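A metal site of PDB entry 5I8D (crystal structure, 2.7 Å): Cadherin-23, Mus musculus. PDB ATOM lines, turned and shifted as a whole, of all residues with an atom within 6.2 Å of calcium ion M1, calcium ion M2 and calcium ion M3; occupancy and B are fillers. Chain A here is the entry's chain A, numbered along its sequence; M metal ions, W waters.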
ATOM      1  N   GLU A  23       7.774  30.093   9.800  1.00  0.00           N
ATOM      2  CA  GLU A  23       8.825  30.262   8.783  1.00  0.00           C
ATOM      3  C   GLU A  23       9.050  28.917   8.043  1.00  0.00           C
ATOM      4  O   GLU A  23       8.623  27.861   8.513  1.00  0.00           O
ATOM      5  CB  GLU A  23      10.140  30.797   9.398  1.00  0.00           C
ATOM      6  CG  GLU A  23      10.861  29.863  10.390  1.00  0.00           C
ATOM      7  CD  GLU A  23      12.260  30.340  10.795  1.00  0.00           C
ATOM      8  OE1 GLU A  23      12.727  29.880  11.861  1.00  0.00           O
ATOM      9  OE2 GLU A  23      12.891  31.155  10.063  1.00  0.00           O
ATOM     10  N   ASN A  24       9.692  28.992   6.876  1.00  0.00           N
ATOM     11  CA  ASN A  24       9.988  27.804   6.043  1.00  0.00           C
ATOM     12  C   ASN A  24       8.706  27.033   5.665  1.00  0.00           C
ATOM     13  O   ASN A  24       8.764  25.831   5.400  1.00  0.00           O
ATOM     14  CB  ASN A  24      10.970  26.835   6.734  1.00  0.00           C
ATOM     15  CG  ASN A  24      12.191  27.532   7.320  1.00  0.00           C
ATOM     16  OD1 ASN A  24      12.778  28.431   6.709  1.00  0.00           O
ATOM     17  ND2 ASN A  24      12.593  27.096   8.526  1.00  0.00           N
ATOM     18  N   ILE A  80      10.244  32.086   3.322  1.00  0.00           N
ATOM     19  CA  ILE A  80       9.976  32.955   4.485  1.00  0.00           C
ATOM     20  C   ILE A  80      10.916  32.564   5.631  1.00  0.00           C
ATOM     21  O   ILE A  80      10.726  31.522   6.259  1.00  0.00           O
ATOM     22  CB  ILE A  80       8.495  32.868   4.961  1.00  0.00           C
ATOM     23  CG1 ILE A  80       7.546  33.268   3.820  1.00  0.00           C
ATOM     24  CG2 ILE A  80       8.279  33.764   6.187  1.00  0.00           C
ATOM     25  CD1 ILE A  80       6.078  33.048   4.129  1.00  0.00           C
ATOM     26  N   ASP A  81      11.913  33.425   5.900  1.00  0.00           N
ATOM     27  CA  ASP A  81      12.976  33.170   6.910  1.00  0.00           C
ATOM     28  C   ASP A  81      12.952  34.209   8.051  1.00  0.00           C
ATOM     29  O   ASP A  81      13.441  35.358   7.887  1.00  0.00           O
ATOM     30  CB  ASP A  81      14.350  33.161   6.223  1.00  0.00           C
ATOM     31  CG  ASP A  81      15.516  33.363   7.195  1.00  0.00           C
ATOM     32  OD1 ASP A  81      15.511  32.751   8.289  1.00  0.00           O
ATOM     33  OD2 ASP A  81      16.438  34.134   6.865  1.00  0.00           O
ATOM     34  N   ARG A  82      12.449  33.790   9.206  1.00  0.00           N
ATOM     35  CA  ARG A  82      12.352  34.673  10.384  1.00  0.00           C
ATOM     36  C   ARG A  82      13.635  35.499  10.640  1.00  0.00           C
ATOM     37  O   ARG A  82      13.580  36.731  10.790  1.00  0.00           O
ATOM     38  CB  ARG A  82      11.983  33.871  11.634  1.00  0.00           C
ATOM     39  CG  ARG A  82      11.450  34.725  12.770  1.00  0.00           C
ATOM     40  CD  ARG A  82      11.453  33.957  14.081  1.00  0.00           C
ATOM     41  NE  ARG A  82      12.806  33.787  14.613  1.00  0.00           N
ATOM     42  CZ  ARG A  82      13.486  34.674  15.341  1.00  0.00           C
ATOM     43  NH1 ARG A  82      14.721  34.380  15.760  1.00  0.00           N
ATOM     44  NH2 ARG A  82      12.956  35.877  15.666  1.00  0.00           N
ATOM     45  N   GLU A  83      14.771  34.809  10.576  1.00  0.00           N
ATOM     46  CA  GLU A  83      16.086  35.412  10.790  1.00  0.00           C
ATOM     47  C   GLU A  83      16.469  36.551   9.815  1.00  0.00           C
ATOM     48  O   GLU A  83      17.497  37.188  10.042  1.00  0.00           O
ATOM     49  CB  GLU A  83      17.188  34.334  10.728  1.00  0.00           C
ATOM     50  CG  GLU A  83      17.277  33.475  11.973  1.00  0.00           C
ATOM     51  CD  GLU A  83      16.072  32.579  12.163  1.00  0.00           C
ATOM     52  OE1 GLU A  83      15.783  31.732  11.278  1.00  0.00           O
ATOM     53  OE2 GLU A  83      15.403  32.707  13.209  1.00  0.00           O
ATOM     54  N   ASP A 114       8.648  31.278  14.917  1.00  0.00           N
ATOM     55  CA  ASP A 114      10.012  30.696  14.894  1.00  0.00           C
ATOM     56  C   ASP A 114      10.033  29.185  14.752  1.00  0.00           C
ATOM     57  O   ASP A 114       9.273  28.462  15.401  1.00  0.00           O
ATOM     58  CB  ASP A 114      10.817  31.083  16.152  1.00  0.00           C
ATOM     59  CG  ASP A 114      12.306  30.671  16.057  1.00  0.00           C
ATOM     60  OD1 ASP A 114      12.960  30.946  15.017  1.00  0.00           O
ATOM     61  OD2 ASP A 114      12.839  30.075  17.019  1.00  0.00           O
ATOM     62  N   ASP A 115      10.968  28.736  13.902  1.00  0.00           N
ATOM     63  CA  ASP A 115      11.280  27.323  13.702  1.00  0.00           C
ATOM     64  C   ASP A 115      12.739  27.132  14.098  1.00  0.00           C
ATOM     65  O   ASP A 115      13.581  27.962  13.792  1.00  0.00           O
ATOM     66  CB  ASP A 115      11.071  26.967  12.234  1.00  0.00           C
ATOM     67  CG  ASP A 115      11.299  25.508  11.925  1.00  0.00           C
ATOM     68  OD1 ASP A 115      11.086  24.652  12.825  1.00  0.00           O
ATOM     69  OD2 ASP A 115      11.675  25.228  10.751  1.00  0.00           O
ATOM     70  N   ASN A 116      13.040  26.029  14.776  1.00  0.00           N
ATOM     71  CA  ASN A 116      14.392  25.757  15.238  1.00  0.00           C
ATOM     72  C   ASN A 116      15.252  25.271  14.073  1.00  0.00           C
ATOM     73  O   ASN A 116      15.514  24.071  13.941  1.00  0.00           O
ATOM     74  CB  ASN A 116      14.361  24.737  16.378  1.00  0.00           C
ATOM     75  CG  ASN A 116      15.693  24.607  17.085  1.00  0.00           C
ATOM     76  OD1 ASN A 116      16.446  25.574  17.207  1.00  0.00           O
ATOM     77  ND2 ASN A 116      16.002  23.410  17.558  1.00  0.00           N
ATOM     78  N   ASP A 117      15.677  26.225  13.226  1.00  0.00           N
ATOM     79  CA  ASP A 117      16.390  25.910  11.975  1.00  0.00           C
ATOM     80  C   ASP A 117      17.844  26.396  11.903  1.00  0.00           C
ATOM     81  O   ASP A 117      18.463  26.372  10.835  1.00  0.00           O
ATOM     82  CB  ASP A 117      15.585  26.402  10.752  1.00  0.00           C
ATOM     83  CG  ASP A 117      15.489  27.911  10.657  1.00  0.00           C
ATOM     84  OD1 ASP A 117      15.403  28.624  11.675  1.00  0.00           O
ATOM     85  OD2 ASP A 117      15.476  28.405   9.513  1.00  0.00           O
ATOM     86  N   ASN A 118      18.377  26.816  13.062  1.00  0.00           N
ATOM     87  CA  ASN A 118      19.779  27.260  13.204  1.00  0.00           C
ATOM     88  C   ASN A 118      20.445  26.466  14.308  1.00  0.00           C
ATOM     89  O   ASN A 118      19.895  26.350  15.402  1.00  0.00           O
ATOM     90  CB  ASN A 118      19.872  28.747  13.547  1.00  0.00           C
ATOM     91  CG  ASN A 118      19.587  29.642  12.355  1.00  0.00           C
ATOM     92  OD1 ASN A 118      20.503  30.067  11.673  1.00  0.00           O
ATOM     93  ND2 ASN A 118      18.317  29.935  12.110  1.00  0.00           N
ATOM     94  N   TRP A 119      21.645  25.961  14.028  1.00  0.00           N
ATOM     95  CA  TRP A 119      22.412  25.155  14.974  1.00  0.00           C
ATOM     96  C   TRP A 119      23.170  26.065  15.960  1.00  0.00           C
ATOM     97  O   TRP A 119      23.694  27.089  15.560  1.00  0.00           O
ATOM     98  CB  TRP A 119      23.432  24.278  14.242  1.00  0.00           C
ATOM     99  CG  TRP A 119      22.885  23.032  13.587  1.00  0.00           C
ATOM    100  CD1 TRP A 119      22.971  21.761  14.069  1.00  0.00           C
ATOM    101  CD2 TRP A 119      22.235  22.938  12.315  1.00  0.00           C
ATOM    102  NE1 TRP A 119      22.388  20.885  13.190  1.00  0.00           N
ATOM    103  CE2 TRP A 119      21.932  21.579  12.107  1.00  0.00           C
ATOM    104  CE3 TRP A 119      21.862  23.877  11.332  1.00  0.00           C
ATOM    105  CZ2 TRP A 119      21.272  21.123  10.947  1.00  0.00           C
ATOM    106  CZ3 TRP A 119      21.210  23.419  10.187  1.00  0.00           C
ATOM    107  CH2 TRP A 119      20.916  22.064  10.002  1.00  0.00           C
ATOM    108  N   PRO A 120      23.228  25.679  17.257  1.00  0.00           N
ATOM    109  CA  PRO A 120      24.261  26.287  18.099  1.00  0.00           C
ATOM    110  C   PRO A 120      25.635  26.115  17.429  1.00  0.00           C
ATOM    111  O   PRO A 120      26.058  24.980  17.195  1.00  0.00           O
ATOM    112  CB  PRO A 120      24.185  25.462  19.394  1.00  0.00           C
ATOM    113  CG  PRO A 120      22.781  24.962  19.444  1.00  0.00           C
ATOM    114  CD  PRO A 120      22.319  24.800  18.026  1.00  0.00           C
ATOM    115  N   ASP A 148      23.554  31.100  18.611  1.00  0.00           N
ATOM    116  CA  ASP A 148      22.406  30.465  17.941  1.00  0.00           C
ATOM    117  C   ASP A 148      21.456  31.568  17.466  1.00  0.00           C
ATOM    118  O   ASP A 148      20.894  32.296  18.294  1.00  0.00           O
ATOM    119  CB  ASP A 148      21.699  29.512  18.929  1.00  0.00           C
ATOM    120  CG  ASP A 148      20.581  28.675  18.280  1.00  0.00           C
ATOM    121  OD1 ASP A 148      19.807  29.193  17.445  1.00  0.00           O
ATOM    122  OD2 ASP A 148      20.450  27.465  18.626  1.00  0.00           O
ATOM    123  N   GLU A 149      21.242  31.675  16.153  1.00  0.00           N
ATOM    124  CA  GLU A 149      20.426  32.762  15.588  1.00  0.00           C
ATOM    125  C   GLU A 149      18.897  32.614  15.809  1.00  0.00           C
ATOM    126  O   GLU A 149      18.143  33.507  15.448  1.00  0.00           O
ATOM    127  CB  GLU A 149      20.701  32.940  14.088  1.00  0.00           C
ATOM    128  CG  GLU A 149      22.166  33.075  13.681  1.00  0.00           C
ATOM    129  CD  GLU A 149      22.973  34.024  14.551  1.00  0.00           C
ATOM    130  OE1 GLU A 149      23.804  33.541  15.357  1.00  0.00           O
ATOM    131  OE2 GLU A 149      22.786  35.258  14.428  1.00  0.00           O
ATOM    132  N   ASP A 150      18.441  31.505  16.376  1.00  0.00           N
ATOM    133  CA  ASP A 150      17.020  31.352  16.725  1.00  0.00           C
ATOM    134  C   ASP A 150      16.694  32.094  18.033  1.00  0.00           C
ATOM    135  O   ASP A 150      17.598  32.597  18.731  1.00  0.00           O
ATOM    136  CB  ASP A 150      16.636  29.869  16.844  1.00  0.00           C
ATOM    137  CG  ASP A 150      16.885  29.090  15.556  1.00  0.00           C
ATOM    138  OD1 ASP A 150      16.675  29.643  14.443  1.00  0.00           O
ATOM    139  OD2 ASP A 150      17.301  27.912  15.672  1.00  0.00           O
ATOM    140  N   SER A 151      15.393  32.142  18.336  1.00  0.00           N
ATOM    141  CA  SER A 151      14.857  32.862  19.503  1.00  0.00           C
ATOM    142  C   SER A 151      14.293  31.880  20.539  1.00  0.00           C
ATOM    143  O   SER A 151      14.382  30.652  20.379  1.00  0.00           O
ATOM    144  CB  SER A 151      13.775  33.850  19.049  1.00  0.00           C
ATOM    145  OG  SER A 151      12.630  33.165  18.551  1.00  0.00           O
ATOM    146  N   LEU A 153      13.273  29.358  23.297  1.00  0.00           N
ATOM    147  CA  LEU A 153      13.906  28.096  23.641  1.00  0.00           C
ATOM    148  C   LEU A 153      14.746  27.542  22.475  1.00  0.00           C
ATOM    149  O   LEU A 153      15.690  26.756  22.687  1.00  0.00           O
ATOM    150  CB  LEU A 153      12.839  27.071  24.086  1.00  0.00           C
ATOM    151  CG  LEU A 153      12.038  27.419  25.361  1.00  0.00           C
ATOM    152  CD1 LEU A 153      10.858  26.471  25.555  1.00  0.00           C
ATOM    153  CD2 LEU A 153      12.901  27.442  26.611  1.00  0.00           C
ATOM    154  N   ASN A 154      14.432  27.988  21.258  1.00  0.00           N
ATOM    155  CA  ASN A 154      15.189  27.570  20.071  1.00  0.00           C
ATOM    156  C   ASN A 154      16.590  28.167  20.026  1.00  0.00           C
ATOM    157  O   ASN A 154      17.465  27.629  19.341  1.00  0.00           O
ATOM    158  CB  ASN A 154      14.428  27.902  18.785  1.00  0.00           C
ATOM    159  CG  ASN A 154      13.070  27.227  18.730  1.00  0.00           C
ATOM    160  OD1 ASN A 154      12.737  26.343  19.523  1.00  0.00           O
ATOM    161  ND2 ASN A 154      12.259  27.634  17.757  1.00  0.00           N
ATOM    162  N   GLY A 155      16.803  29.284  20.747  1.00  0.00           N
ATOM    163  CA  GLY A 155      18.126  29.915  20.890  1.00  0.00           C
ATOM    164  C   GLY A 155      18.814  29.826  22.249  1.00  0.00           C
ATOM    165  O   GLY A 155      19.925  30.321  22.403  1.00  0.00           O
ATOM    166  N   LEU A 157      20.746  28.032  25.242  1.00  0.00           N
ATOM    167  CA  LEU A 157      21.728  26.938  25.172  1.00  0.00           C
ATOM    168  C   LEU A 157      22.105  26.351  26.542  1.00  0.00           C
ATOM    169  O   LEU A 157      22.396  27.093  27.486  1.00  0.00           O
ATOM    170  CB  LEU A 157      22.995  27.427  24.456  1.00  0.00           C
ATOM    171  CG  LEU A 157      22.743  28.211  23.155  1.00  0.00           C
ATOM    172  CD1 LEU A 157      24.033  28.736  22.512  1.00  0.00           C
ATOM    173  CD2 LEU A 157      21.939  27.360  22.176  1.00  0.00           C
ATOM    174  N   ASP A 201      20.589  23.469  22.127  1.00  0.00           N
ATOM    175  CA  ASP A 201      19.415  24.360  22.297  1.00  0.00           C
ATOM    176  C   ASP A 201      18.180  23.628  22.851  1.00  0.00           C
ATOM    177  O   ASP A 201      18.215  22.409  23.040  1.00  0.00           O
ATOM    178  CB  ASP A 201      19.106  25.168  21.011  1.00  0.00           C
ATOM    179  CG  ASP A 201      18.482  24.331  19.890  1.00  0.00           C
ATOM    180  OD1 ASP A 201      17.810  23.317  20.164  1.00  0.00           O
ATOM    181  OD2 ASP A 201      18.654  24.726  18.715  1.00  0.00           O
ATOM    182  N   LEU A 207      18.714  20.991  18.722  1.00  0.00           N
ATOM    183  CA  LEU A 207      19.932  20.995  17.894  1.00  0.00           C
ATOM    184  C   LEU A 207      21.146  21.311  18.763  1.00  0.00           C
ATOM    185  O   LEU A 207      21.063  22.113  19.723  1.00  0.00           O
ATOM    186  CB  LEU A 207      19.858  22.010  16.733  1.00  0.00           C
ATOM    187  CG  LEU A 207      18.834  21.790  15.601  1.00  0.00           C
ATOM    188  CD1 LEU A 207      18.910  22.898  14.565  1.00  0.00           C
ATOM    189  CD2 LEU A 207      19.037  20.435  14.930  1.00  0.00           C
HETATM  190 CA    CA M   1      18.559  26.595  17.295  1.00  0.00          CA
HETATM  191 CA    CA M   2      14.589  30.219  13.219  1.00  0.00          CA
HETATM  192 CA    CA M   3      15.098  30.612   9.099  1.00  0.00          CA
HETATM  193  O   HOH W   1      17.348  30.623   9.244  1.00  0.00           O
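OE1 of Glu 23 is bound to calcium ion M2, at 2.3 Å.
OD1 of Asp 117 is bound to calcium ion M2, at 2.4 Å.
Calcium ion M2 is bound by OD1 of Asp 150, at 2.5 Å.
OD1 of Asp 114 is bound to calcium ion M2, 2.5 Å away.
O of Asp 115 is bound to calcium ion M2, at 2.5 Å.
Calcium ion M2 is bound by the side-chain carboxylate (OE2) of Glu 83, at 2.6 Å.
The side-chain carboxylate (OE1) of Glu 83 is bound to calcium ion M2.
Of the 23 residues printed, 7 come within 4 Å of calcium ion M2.
The nearest printed residue that does not touch calcium ion M2 is Arg 82 (4.2 Å).
The side-chain carboxylate (OD2) of Asp 114 is in hydrogen-bond range of the side-chain hydroxyl (OG) of Ser 151 (3.5 Å).
NE of Arg 82 lies close to OD1 of Asp 114.
The side-chain carboxylate (OE1) of Glu 83 sits close to the side-chain amide nitrogen (ND2) of Asn 118 (3.2 Å).
The side-chain carboxylate (OD2) of Asp 117 lies close to the side-chain amide nitrogen (ND2) of Asn 24.
N of Asn 24 sits at hydrogen-bond distance from O of Ile 80, at 2.8 Å.
OD2 of Asp 114 is in hydrogen-bond range of ND2 of Asn 154 (2.6 Å).
OE2 of Glu 83 sits close to NH1 of Arg 82 (3.1 Å).
The backbone carbonyl oxygen (O) of Leu 207 sits at hydrogen-bond distance from the backbone NH (N) of Asp 201, at 2.8 Å.
Calcium ion M3 is bound by water W1 (2.3 Å), the side-chain carboxylate of Asp 117 (2.3 Å), the side-chain carboxylate of Asp 81 (2.3 Å), the side-chain carboxylate of Glu 23 (2.5 Å) and the side-chain carboxylate of Glu 83 (2.5 Å).
Calcium ion M3 has five donor atoms within binding distance.
The backbone carbonyl oxygen (O) of Asn 118 binds calcium ion M1 (2.3 Å).
Calcium ion M1 is bound by OD1 of Asn 116 (2.3 Å).
The side-chain carboxylate (OD2) of Asp 201 is bound to calcium ion M1 (2.3 Å).
OD2 of Asp 150 binds calcium ion M1.
OD2 of Asp 148 is bound to calcium ion M1, at 2.5 Å.
Calcium ion M1 is bound by the backbone carbonyl oxygen (O) of Asn 154 (2.5 Å).
Calcium ion M1 is bound by OD1 of Asp 148 (2.9 Å).
Calcium ion M1 has seven donor atoms within binding distance.
The nearest printed residue that does not touch calcium ion M1 is Pro 120 (4.2 Å).
Asn 24 touches calcium ion M3 (OD1 to CA, 3.98 Å).
Of the 23 residues printed, 5 come within 4 Å of calcium ion M3.
Along chain A the residues within 4 Å of calcium ion M3 span positions 23 to 117.
The nearest printed residue that does not touch calcium ion M3 is Arg 82 (4.1 Å).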
